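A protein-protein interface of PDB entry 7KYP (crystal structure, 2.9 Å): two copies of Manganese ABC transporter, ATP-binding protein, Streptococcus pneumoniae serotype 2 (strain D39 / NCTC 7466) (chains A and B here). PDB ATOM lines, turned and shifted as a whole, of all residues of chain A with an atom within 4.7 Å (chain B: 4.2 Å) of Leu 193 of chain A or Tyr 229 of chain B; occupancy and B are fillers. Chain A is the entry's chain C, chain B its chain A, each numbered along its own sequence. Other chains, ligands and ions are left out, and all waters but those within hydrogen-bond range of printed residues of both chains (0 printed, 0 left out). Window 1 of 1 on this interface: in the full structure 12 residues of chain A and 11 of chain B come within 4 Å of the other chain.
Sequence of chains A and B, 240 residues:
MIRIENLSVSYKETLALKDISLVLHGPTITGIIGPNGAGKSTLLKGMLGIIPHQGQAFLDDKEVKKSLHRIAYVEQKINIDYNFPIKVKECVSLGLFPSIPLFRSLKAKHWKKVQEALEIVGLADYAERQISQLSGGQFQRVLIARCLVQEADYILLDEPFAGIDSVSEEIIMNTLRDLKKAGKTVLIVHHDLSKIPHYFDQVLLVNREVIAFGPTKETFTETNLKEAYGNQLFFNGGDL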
ATOM      1  N   ILE A  33     -17.857 -22.343 -10.025  1.00  0.00           N
ATOM      2  CA  ILE A  33     -17.155 -22.357 -11.311  1.00  0.00           C
ATOM      3  C   ILE A  33     -16.746 -20.952 -11.744  1.00  0.00           C
ATOM      4  O   ILE A  33     -17.227 -19.953 -11.206  1.00  0.00           O
ATOM      5  CB  ILE A  33     -18.005 -23.011 -12.427  1.00  0.00           C
ATOM      6  CG1 ILE A  33     -19.407 -22.394 -12.485  1.00  0.00           C
ATOM      7  CG2 ILE A  33     -18.096 -24.512 -12.208  1.00  0.00           C
ATOM      8  CD1 ILE A  33     -20.169 -22.712 -13.754  1.00  0.00           C
ATOM      9  N   HIS A 190     -15.045 -26.310  -8.652  1.00  0.00           N
ATOM     10  CA  HIS A 190     -14.772 -27.126  -9.836  1.00  0.00           C
ATOM     11  C   HIS A 190     -13.634 -26.516 -10.655  1.00  0.00           C
ATOM     12  O   HIS A 190     -13.518 -25.296 -10.760  1.00  0.00           O
ATOM     13  CB  HIS A 190     -16.038 -27.279 -10.684  1.00  0.00           C
ATOM     14  CG  HIS A 190     -16.026 -28.477 -11.582  1.00  0.00           C
ATOM     15  ND1 HIS A 190     -15.648 -29.729 -11.149  1.00  0.00           N
ATOM     16  CD2 HIS A 190     -16.366 -28.619 -12.886  1.00  0.00           C
ATOM     17  CE1 HIS A 190     -15.743 -30.587 -12.149  1.00  0.00           C
ATOM     18  NE2 HIS A 190     -16.179 -29.939 -13.214  1.00  0.00           N
ATOM     19  N   ASP A 192     -12.927 -26.886 -13.981  1.00  0.00           N
ATOM     20  CA  ASP A 192     -13.258 -26.493 -15.351  1.00  0.00           C
ATOM     21  C   ASP A 192     -14.781 -26.339 -15.508  1.00  0.00           C
ATOM     22  O   ASP A 192     -15.461 -25.990 -14.543  1.00  0.00           O
ATOM     23  CB  ASP A 192     -12.656 -27.506 -16.340  1.00  0.00           C
ATOM     24  CG  ASP A 192     -13.198 -28.918 -16.155  1.00  0.00           C
ATOM     25  OD1 ASP A 192     -14.054 -29.137 -15.271  1.00  0.00           O
ATOM     26  OD2 ASP A 192     -12.753 -29.818 -16.899  1.00  0.00           O
ATOM     27  N   LEU A 193     -15.309 -26.570 -16.712  1.00  0.00           N
ATOM     28  CA  LEU A 193     -16.754 -26.558 -16.949  1.00  0.00           C
ATOM     29  C   LEU A 193     -17.220 -27.918 -17.470  1.00  0.00           C
ATOM     30  O   LEU A 193     -17.970 -27.999 -18.447  1.00  0.00           O
ATOM     31  CB  LEU A 193     -17.116 -25.454 -17.948  1.00  0.00           C
ATOM     32  CG  LEU A 193     -16.755 -24.024 -17.545  1.00  0.00           C
ATOM     33  CD1 LEU A 193     -17.008 -23.072 -18.704  1.00  0.00           C
ATOM     34  CD2 LEU A 193     -17.536 -23.593 -16.315  1.00  0.00           C
ATOM     35  N   SER A 194     -16.774 -28.983 -16.806  1.00  0.00           N
ATOM     36  CA  SER A 194     -17.088 -30.349 -17.220  1.00  0.00           C
ATOM     37  C   SER A 194     -18.217 -30.934 -16.377  1.00  0.00           C
ATOM     38  O   SER A 194     -18.136 -30.939 -15.149  1.00  0.00           O
ATOM     39  CB  SER A 194     -15.848 -31.235 -17.100  1.00  0.00           C
ATOM     40  OG  SER A 194     -15.462 -31.396 -15.746  1.00  0.00           O
ATOM     41  N   LYS A 195     -19.260 -31.421 -17.047  1.00  0.00           N
ATOM     42  CA  LYS A 195     -20.369 -32.131 -16.400  1.00  0.00           C
ATOM     43  C   LYS A 195     -21.038 -31.315 -15.290  1.00  0.00           C
ATOM     44  O   LYS A 195     -21.280 -31.824 -14.194  1.00  0.00           O
ATOM     45  CB  LYS A 195     -19.887 -33.471 -15.833  1.00  0.00           C
ATOM     46  CG  LYS A 195     -18.971 -34.277 -16.738  1.00  0.00           C
ATOM     47  CD  LYS A 195     -18.725 -35.652 -16.140  1.00  0.00           C
ATOM     48  CE  LYS A 195     -17.541 -36.347 -16.785  1.00  0.00           C
ATOM     49  NZ  LYS A 195     -17.352 -37.720 -16.241  1.00  0.00           N
ATOM     50  N   ILE A 196     -21.351 -30.056 -15.583  1.00  0.00           N
ATOM     51  CA  ILE A 196     -21.912 -29.145 -14.579  1.00  0.00           C
ATOM     52  C   ILE A 196     -23.264 -29.613 -14.018  1.00  0.00           C
ATOM     53  O   ILE A 196     -23.432 -29.660 -12.799  1.00  0.00           O
ATOM     54  CB  ILE A 196     -22.003 -27.693 -15.113  1.00  0.00           C
ATOM     55  CG1 ILE A 196     -20.599 -27.147 -15.420  1.00  0.00           C
ATOM     56  CG2 ILE A 196     -22.723 -26.785 -14.123  1.00  0.00           C
ATOM     57  CD1 ILE A 196     -19.612 -27.239 -14.274  1.00  0.00           C
ATOM     58  N   PHE A 220     -26.719 -21.758 -15.251  1.00  0.00           N
ATOM     59  CA  PHE A 220     -25.656 -22.208 -16.151  1.00  0.00           C
ATOM     60  C   PHE A 220     -26.080 -21.970 -17.602  1.00  0.00           C
ATOM     61  O   PHE A 220     -26.494 -22.893 -18.306  1.00  0.00           O
ATOM     62  CB  PHE A 220     -25.328 -23.686 -15.901  1.00  0.00           C
ATOM     63  CG  PHE A 220     -24.110 -24.171 -16.634  1.00  0.00           C
ATOM     64  CD1 PHE A 220     -22.860 -23.633 -16.361  1.00  0.00           C
ATOM     65  CD2 PHE A 220     -24.210 -25.171 -17.592  1.00  0.00           C
ATOM     66  CE1 PHE A 220     -21.734 -24.077 -17.033  1.00  0.00           C
ATOM     67  CE2 PHE A 220     -23.088 -25.621 -18.265  1.00  0.00           C
ATOM     68  CZ  PHE A 220     -21.848 -25.073 -17.988  1.00  0.00           C
ATOM     69  N   LEU A 225     -22.007 -17.321 -18.625  1.00  0.00           N
ATOM     70  CA  LEU A 225     -20.646 -17.788 -18.899  1.00  0.00           C
ATOM     71  C   LEU A 225     -19.839 -16.759 -19.689  1.00  0.00           C
ATOM     72  O   LEU A 225     -18.668 -16.522 -19.387  1.00  0.00           O
ATOM     73  CB  LEU A 225     -20.669 -19.121 -19.654  1.00  0.00           C
ATOM     74  CG  LEU A 225     -21.136 -20.344 -18.860  1.00  0.00           C
ATOM     75  CD1 LEU A 225     -21.314 -21.539 -19.785  1.00  0.00           C
ATOM     76  CD2 LEU A 225     -20.161 -20.672 -17.737  1.00  0.00           C
ATOM     77  N   TYR A 229     -16.424 -15.398 -18.130  1.00  0.00           N
ATOM     78  CA  TYR A 229     -15.171 -15.707 -18.827  1.00  0.00           C
ATOM     79  C   TYR A 229     -14.743 -14.609 -19.804  1.00  0.00           C
ATOM     80  O   TYR A 229     -13.548 -14.372 -19.990  1.00  0.00           O
ATOM     81  CB  TYR A 229     -15.281 -17.052 -19.554  1.00  0.00           C
ATOM     82  CG  TYR A 229     -15.202 -18.245 -18.627  1.00  0.00           C
ATOM     83  CD1 TYR A 229     -16.299 -18.629 -17.857  1.00  0.00           C
ATOM     84  CD2 TYR A 229     -14.030 -18.988 -18.515  1.00  0.00           C
ATOM     85  CE1 TYR A 229     -16.228 -19.720 -17.005  1.00  0.00           C
ATOM     86  CE2 TYR A 229     -13.951 -20.080 -17.667  1.00  0.00           C
ATOM     87  CZ  TYR A 229     -15.052 -20.441 -16.914  1.00  0.00           C
ATOM     88  OH  TYR A 229     -14.974 -21.526 -16.071  1.00  0.00           O
ATOM     89  N   GLY B  34      -7.741 -19.848 -24.145  1.00  0.00           N
ATOM     90  CA  GLY B  34      -8.094 -21.085 -23.452  1.00  0.00           C
ATOM     91  C   GLY B  34      -7.997 -20.929 -21.945  1.00  0.00           C
ATOM     92  O   GLY B  34      -7.694 -19.840 -21.453  1.00  0.00           O
ATOM     93  N   PRO B  35      -8.260 -22.018 -21.198  1.00  0.00           N
ATOM     94  CA  PRO B  35      -8.182 -21.975 -19.735  1.00  0.00           C
ATOM     95  C   PRO B  35      -6.792 -21.595 -19.226  1.00  0.00           C
ATOM     96  O   PRO B  35      -5.786 -22.045 -19.780  1.00  0.00           O
ATOM     97  CB  PRO B  35      -8.532 -23.409 -19.317  1.00  0.00           C
ATOM     98  CG  PRO B  35      -9.292 -23.974 -20.465  1.00  0.00           C
ATOM     99  CD  PRO B  35      -8.708 -23.334 -21.687  1.00  0.00           C
ATOM    100  N   LEU B 193     -11.341 -13.907 -22.518  1.00  0.00           N
ATOM    101  CA  LEU B 193     -12.010 -13.969 -23.816  1.00  0.00           C
ATOM    102  C   LEU B 193     -12.667 -12.622 -24.124  1.00  0.00           C
ATOM    103  O   LEU B 193     -13.851 -12.556 -24.461  1.00  0.00           O
ATOM    104  CB  LEU B 193     -13.049 -15.095 -23.822  1.00  0.00           C
ATOM    105  CG  LEU B 193     -12.526 -16.500 -23.503  1.00  0.00           C
ATOM    106  CD1 LEU B 193     -13.684 -17.459 -23.274  1.00  0.00           C
ATOM    107  CD2 LEU B 193     -11.618 -17.013 -24.610  1.00  0.00           C
ATOM    108  N   LEU B 225     -15.041 -23.322 -28.123  1.00  0.00           N
ATOM    109  CA  LEU B 225     -14.776 -22.800 -26.781  1.00  0.00           C
ATOM    110  C   LEU B 225     -15.238 -23.754 -25.682  1.00  0.00           C
ATOM    111  O   LEU B 225     -14.492 -24.024 -24.741  1.00  0.00           O
ATOM    112  CB  LEU B 225     -15.440 -21.432 -26.585  1.00  0.00           C
ATOM    113  CG  LEU B 225     -14.831 -20.252 -27.346  1.00  0.00           C
ATOM    114  CD1 LEU B 225     -15.647 -18.992 -27.099  1.00  0.00           C
ATOM    115  CD2 LEU B 225     -13.377 -20.037 -26.954  1.00  0.00           C
ATOM    116  N   LYS B 226     -16.459 -24.269 -25.806  1.00  0.00           N
ATOM    117  CA  LYS B 226     -17.012 -25.156 -24.781  1.00  0.00           C
ATOM    118  C   LYS B 226     -16.313 -26.521 -24.748  1.00  0.00           C
ATOM    119  O   LYS B 226     -16.318 -27.188 -23.715  1.00  0.00           O
ATOM    120  CB  LYS B 226     -18.533 -25.301 -24.931  1.00  0.00           C
ATOM    121  CG  LYS B 226     -19.020 -26.256 -26.014  1.00  0.00           C
ATOM    122  CD  LYS B 226     -20.540 -26.396 -26.016  1.00  0.00           C
ATOM    123  CE  LYS B 226     -21.272 -25.064 -25.891  1.00  0.00           C
ATOM    124  NZ  LYS B 226     -22.739 -25.208 -26.091  1.00  0.00           N
ATOM    125  N   GLU B 227     -15.712 -26.927 -25.864  1.00  0.00           N
ATOM    126  CA  GLU B 227     -14.866 -28.122 -25.887  1.00  0.00           C
ATOM    127  C   GLU B 227     -13.568 -27.887 -25.111  1.00  0.00           C
ATOM    128  O   GLU B 227     -13.090 -28.777 -24.407  1.00  0.00           O
ATOM    129  CB  GLU B 227     -14.548 -28.540 -27.328  1.00  0.00           C
ATOM    130  CG  GLU B 227     -13.625 -29.747 -27.434  1.00  0.00           C
ATOM    131  CD  GLU B 227     -13.592 -30.352 -28.825  1.00  0.00           C
ATOM    132  OE1 GLU B 227     -14.669 -30.718 -29.346  1.00  0.00           O
ATOM    133  OE2 GLU B 227     -12.486 -30.474 -29.395  1.00  0.00           O
ATOM    134  N   ALA B 228     -13.004 -26.687 -25.249  1.00  0.00           N
ATOM    135  CA  ALA B 228     -11.766 -26.324 -24.559  1.00  0.00           C
ATOM    136  C   ALA B 228     -11.992 -26.146 -23.059  1.00  0.00           C
ATOM    137  O   ALA B 228     -11.394 -26.854 -22.249  1.00  0.00           O
ATOM    138  CB  ALA B 228     -11.178 -25.055 -25.160  1.00  0.00           C
ATOM    139  N   TYR B 229     -12.870 -25.212 -22.695  1.00  0.00           N
ATOM    140  CA  TYR B 229     -13.147 -24.913 -21.286  1.00  0.00           C
ATOM    141  C   TYR B 229     -13.923 -26.031 -20.580  1.00  0.00           C
ATOM    142  O   TYR B 229     -13.846 -26.165 -19.359  1.00  0.00           O
ATOM    143  CB  TYR B 229     -13.888 -23.579 -21.151  1.00  0.00           C
ATOM    144  CG  TYR B 229     -13.001 -22.376 -21.381  1.00  0.00           C
ATOM    145  CD1 TYR B 229     -12.736 -21.913 -22.667  1.00  0.00           C
ATOM    146  CD2 TYR B 229     -12.419 -21.703 -20.309  1.00  0.00           C
ATOM    147  CE1 TYR B 229     -11.921 -20.814 -22.881  1.00  0.00           C
ATOM    148  CE2 TYR B 229     -11.603 -20.602 -20.513  1.00  0.00           C
ATOM    149  CZ  TYR B 229     -11.357 -20.162 -21.801  1.00  0.00           C
ATOM    150  OH  TYR B 229     -10.548 -19.070 -22.010  1.00  0.00           O
ATOM    151  N   GLY B 230     -14.670 -26.821 -21.348  1.00  0.00           N
ATOM    152  CA  GLY B 230     -15.354 -27.998 -20.816  1.00  0.00           C
ATOM    153  C   GLY B 230     -14.465 -29.228 -20.757  1.00  0.00           C
ATOM    154  O   GLY B 230     -14.822 -30.220 -20.124  1.00  0.00           O
ATOM    155  N   ASN B 231     -13.317 -29.166 -21.433  1.00  0.00           N
ATOM    156  CA  ASN B 231     -12.321 -30.240 -21.429  1.00  0.00           C
ATOM    157  C   ASN B 231     -12.870 -31.515 -22.077  1.00  0.00           C
ATOM    158  O   ASN B 231     -12.738 -32.614 -21.534  1.00  0.00           O
ATOM    159  CB  ASN B 231     -11.820 -30.508 -19.999  1.00  0.00           C
ATOM    160  CG  ASN B 231     -10.495 -31.252 -19.966  1.00  0.00           C
ATOM    161  OD1 ASN B 231      -9.614 -31.017 -20.794  1.00  0.00           O
ATOM    162  ND2 ASN B 231     -10.346 -32.148 -18.998  1.00  0.00           N
ATOM    163  N   PHE B 234     -18.316 -31.050 -22.044  1.00  0.00           N
ATOM    164  CA  PHE B 234     -19.255 -29.968 -21.749  1.00  0.00           C
ATOM    165  C   PHE B 234     -20.698 -30.448 -21.865  1.00  0.00           C
ATOM    166  O   PHE B 234     -21.076 -31.071 -22.858  1.00  0.00           O
ATOM    167  CB  PHE B 234     -19.027 -28.784 -22.687  1.00  0.00           C
ATOM    168  CG  PHE B 234     -19.654 -27.503 -22.209  1.00  0.00           C
ATOM    169  CD1 PHE B 234     -20.981 -27.212 -22.498  1.00  0.00           C
ATOM    170  CD2 PHE B 234     -18.917 -26.587 -21.470  1.00  0.00           C
ATOM    171  CE1 PHE B 234     -21.561 -26.032 -22.060  1.00  0.00           C
ATOM    172  CE2 PHE B 234     -19.491 -25.405 -21.030  1.00  0.00           C
ATOM    173  CZ  PHE B 234     -20.815 -25.127 -21.325  1.00  0.00           C
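N of Leu 193 of chain B is in hydrogen-bond range of O of Tyr 229 of chain A (3.4 Å).
The backbone carbonyl oxygen (O) of Tyr 229 of chain B is in hydrogen-bond range of the backbone NH (N) of Leu 193 of chain A (3.1 Å).
The side-chain hydroxyl of Tyr 229 of chain B is in hydrogen-bond range of the backbone carbonyl oxygen of Gly 34 of chain B (3.0 Å).
NE2 of His 190 of chain A sits at hydrogen-bond distance from OD1 of Asp 192 of chain A (3.1 Å).
NE2 of His 190 of chain A is in hydrogen-bond range of O of Ser 194 of chain A (2.9 Å).
The side-chain carboxylate (OD1) of Asp 192 of chain A lies within hydrogen-bond range of the side-chain hydroxyl (OG) of Ser 194 of chain A.
Among the printed residues, pairs that only touch across the chains: Asp 192 of chain A with Asn 231 of chain B (3.3 Å), Ser 194 of chain A with Gly 230 of chain B (3.4 Å), Tyr 229 of chain A with Tyr 229 of chain B (3.5 Å), Leu 193 of chain A with Phe 234 of chain B (3.5 Å), Phe 220 of chain A with Phe 234 of chain B (3.5 Å), Asp 192 of chain A with Tyr 229 of chain B (3.5 Å), Leu 193 of chain A with Gly 230 of chain B (3.5 Å), Asp 192 of chain A with Gly 230 of chain B (3.9 Å) and Leu 225 of chain A with Phe 234 of chain B (3.9 Å).
Ile 33 of chain A touches none of the printed residues of chain B.
His 190 of chain A touches none of the printed residues of chain B.
Of the printed residues of chain B, Asp 192 of chain A touches Tyr 229 (3.5 Å), Gly 230 (3.9 Å) and Asn 231 (3.3 Å).
Of chain B, only Tyr 229 (3.1 Å), Gly 230 (3.5 Å) and Phe 234 (3.5 Å) come within 4 Å of Leu 193 of chain A.
Of the printed residues of chain B, Phe 220 of chain A touches Phe 234 (3.5 Å).
Printed residues of chain B within 4 Å of Leu 225 of chain A: Phe 234.
Of chain A, only Asp 192 (3.5 Å), Leu 193 (3.1 Å) and Tyr 229 (3.5 Å) come within 4 Å of Tyr 229 of chain B.
Printed residues of chain A within 4 Å of Asn 231 of chain B: Asp 192 (3.3 Å).
The nearest printed residue of chain B that does not touch Leu 193 of chain A is Lys 226 of chain B (5.6 Å).
Printed residues of chain B that touch a printed residue of chain A: Leu 193, Tyr 229, Gly 230, Asn 231 and Phe 234.
Hydrophobic or aromatic side chains of chain B within 4 Å of the printed part of chain A: Leu 193, Tyr 229 and Phe 234.
Of the 10 printed residues of chain A, 6 touch a printed residue of chain B.
Among the printed residues, 11 pairs touch across the chains.
Leu 193 of chain A touches Tyr 229 of chain B, and with the chains exchanged Tyr 229 of chain A touches Leu 193 of chain B.
Tyr 229 of chain B touches its own counterpart, Tyr 229 of chain A.
3 positions are printed for both chains.
Of the 11 pairs that touch across the chains among the printed residues, 3 have their exchanged pair printed and touching as well.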
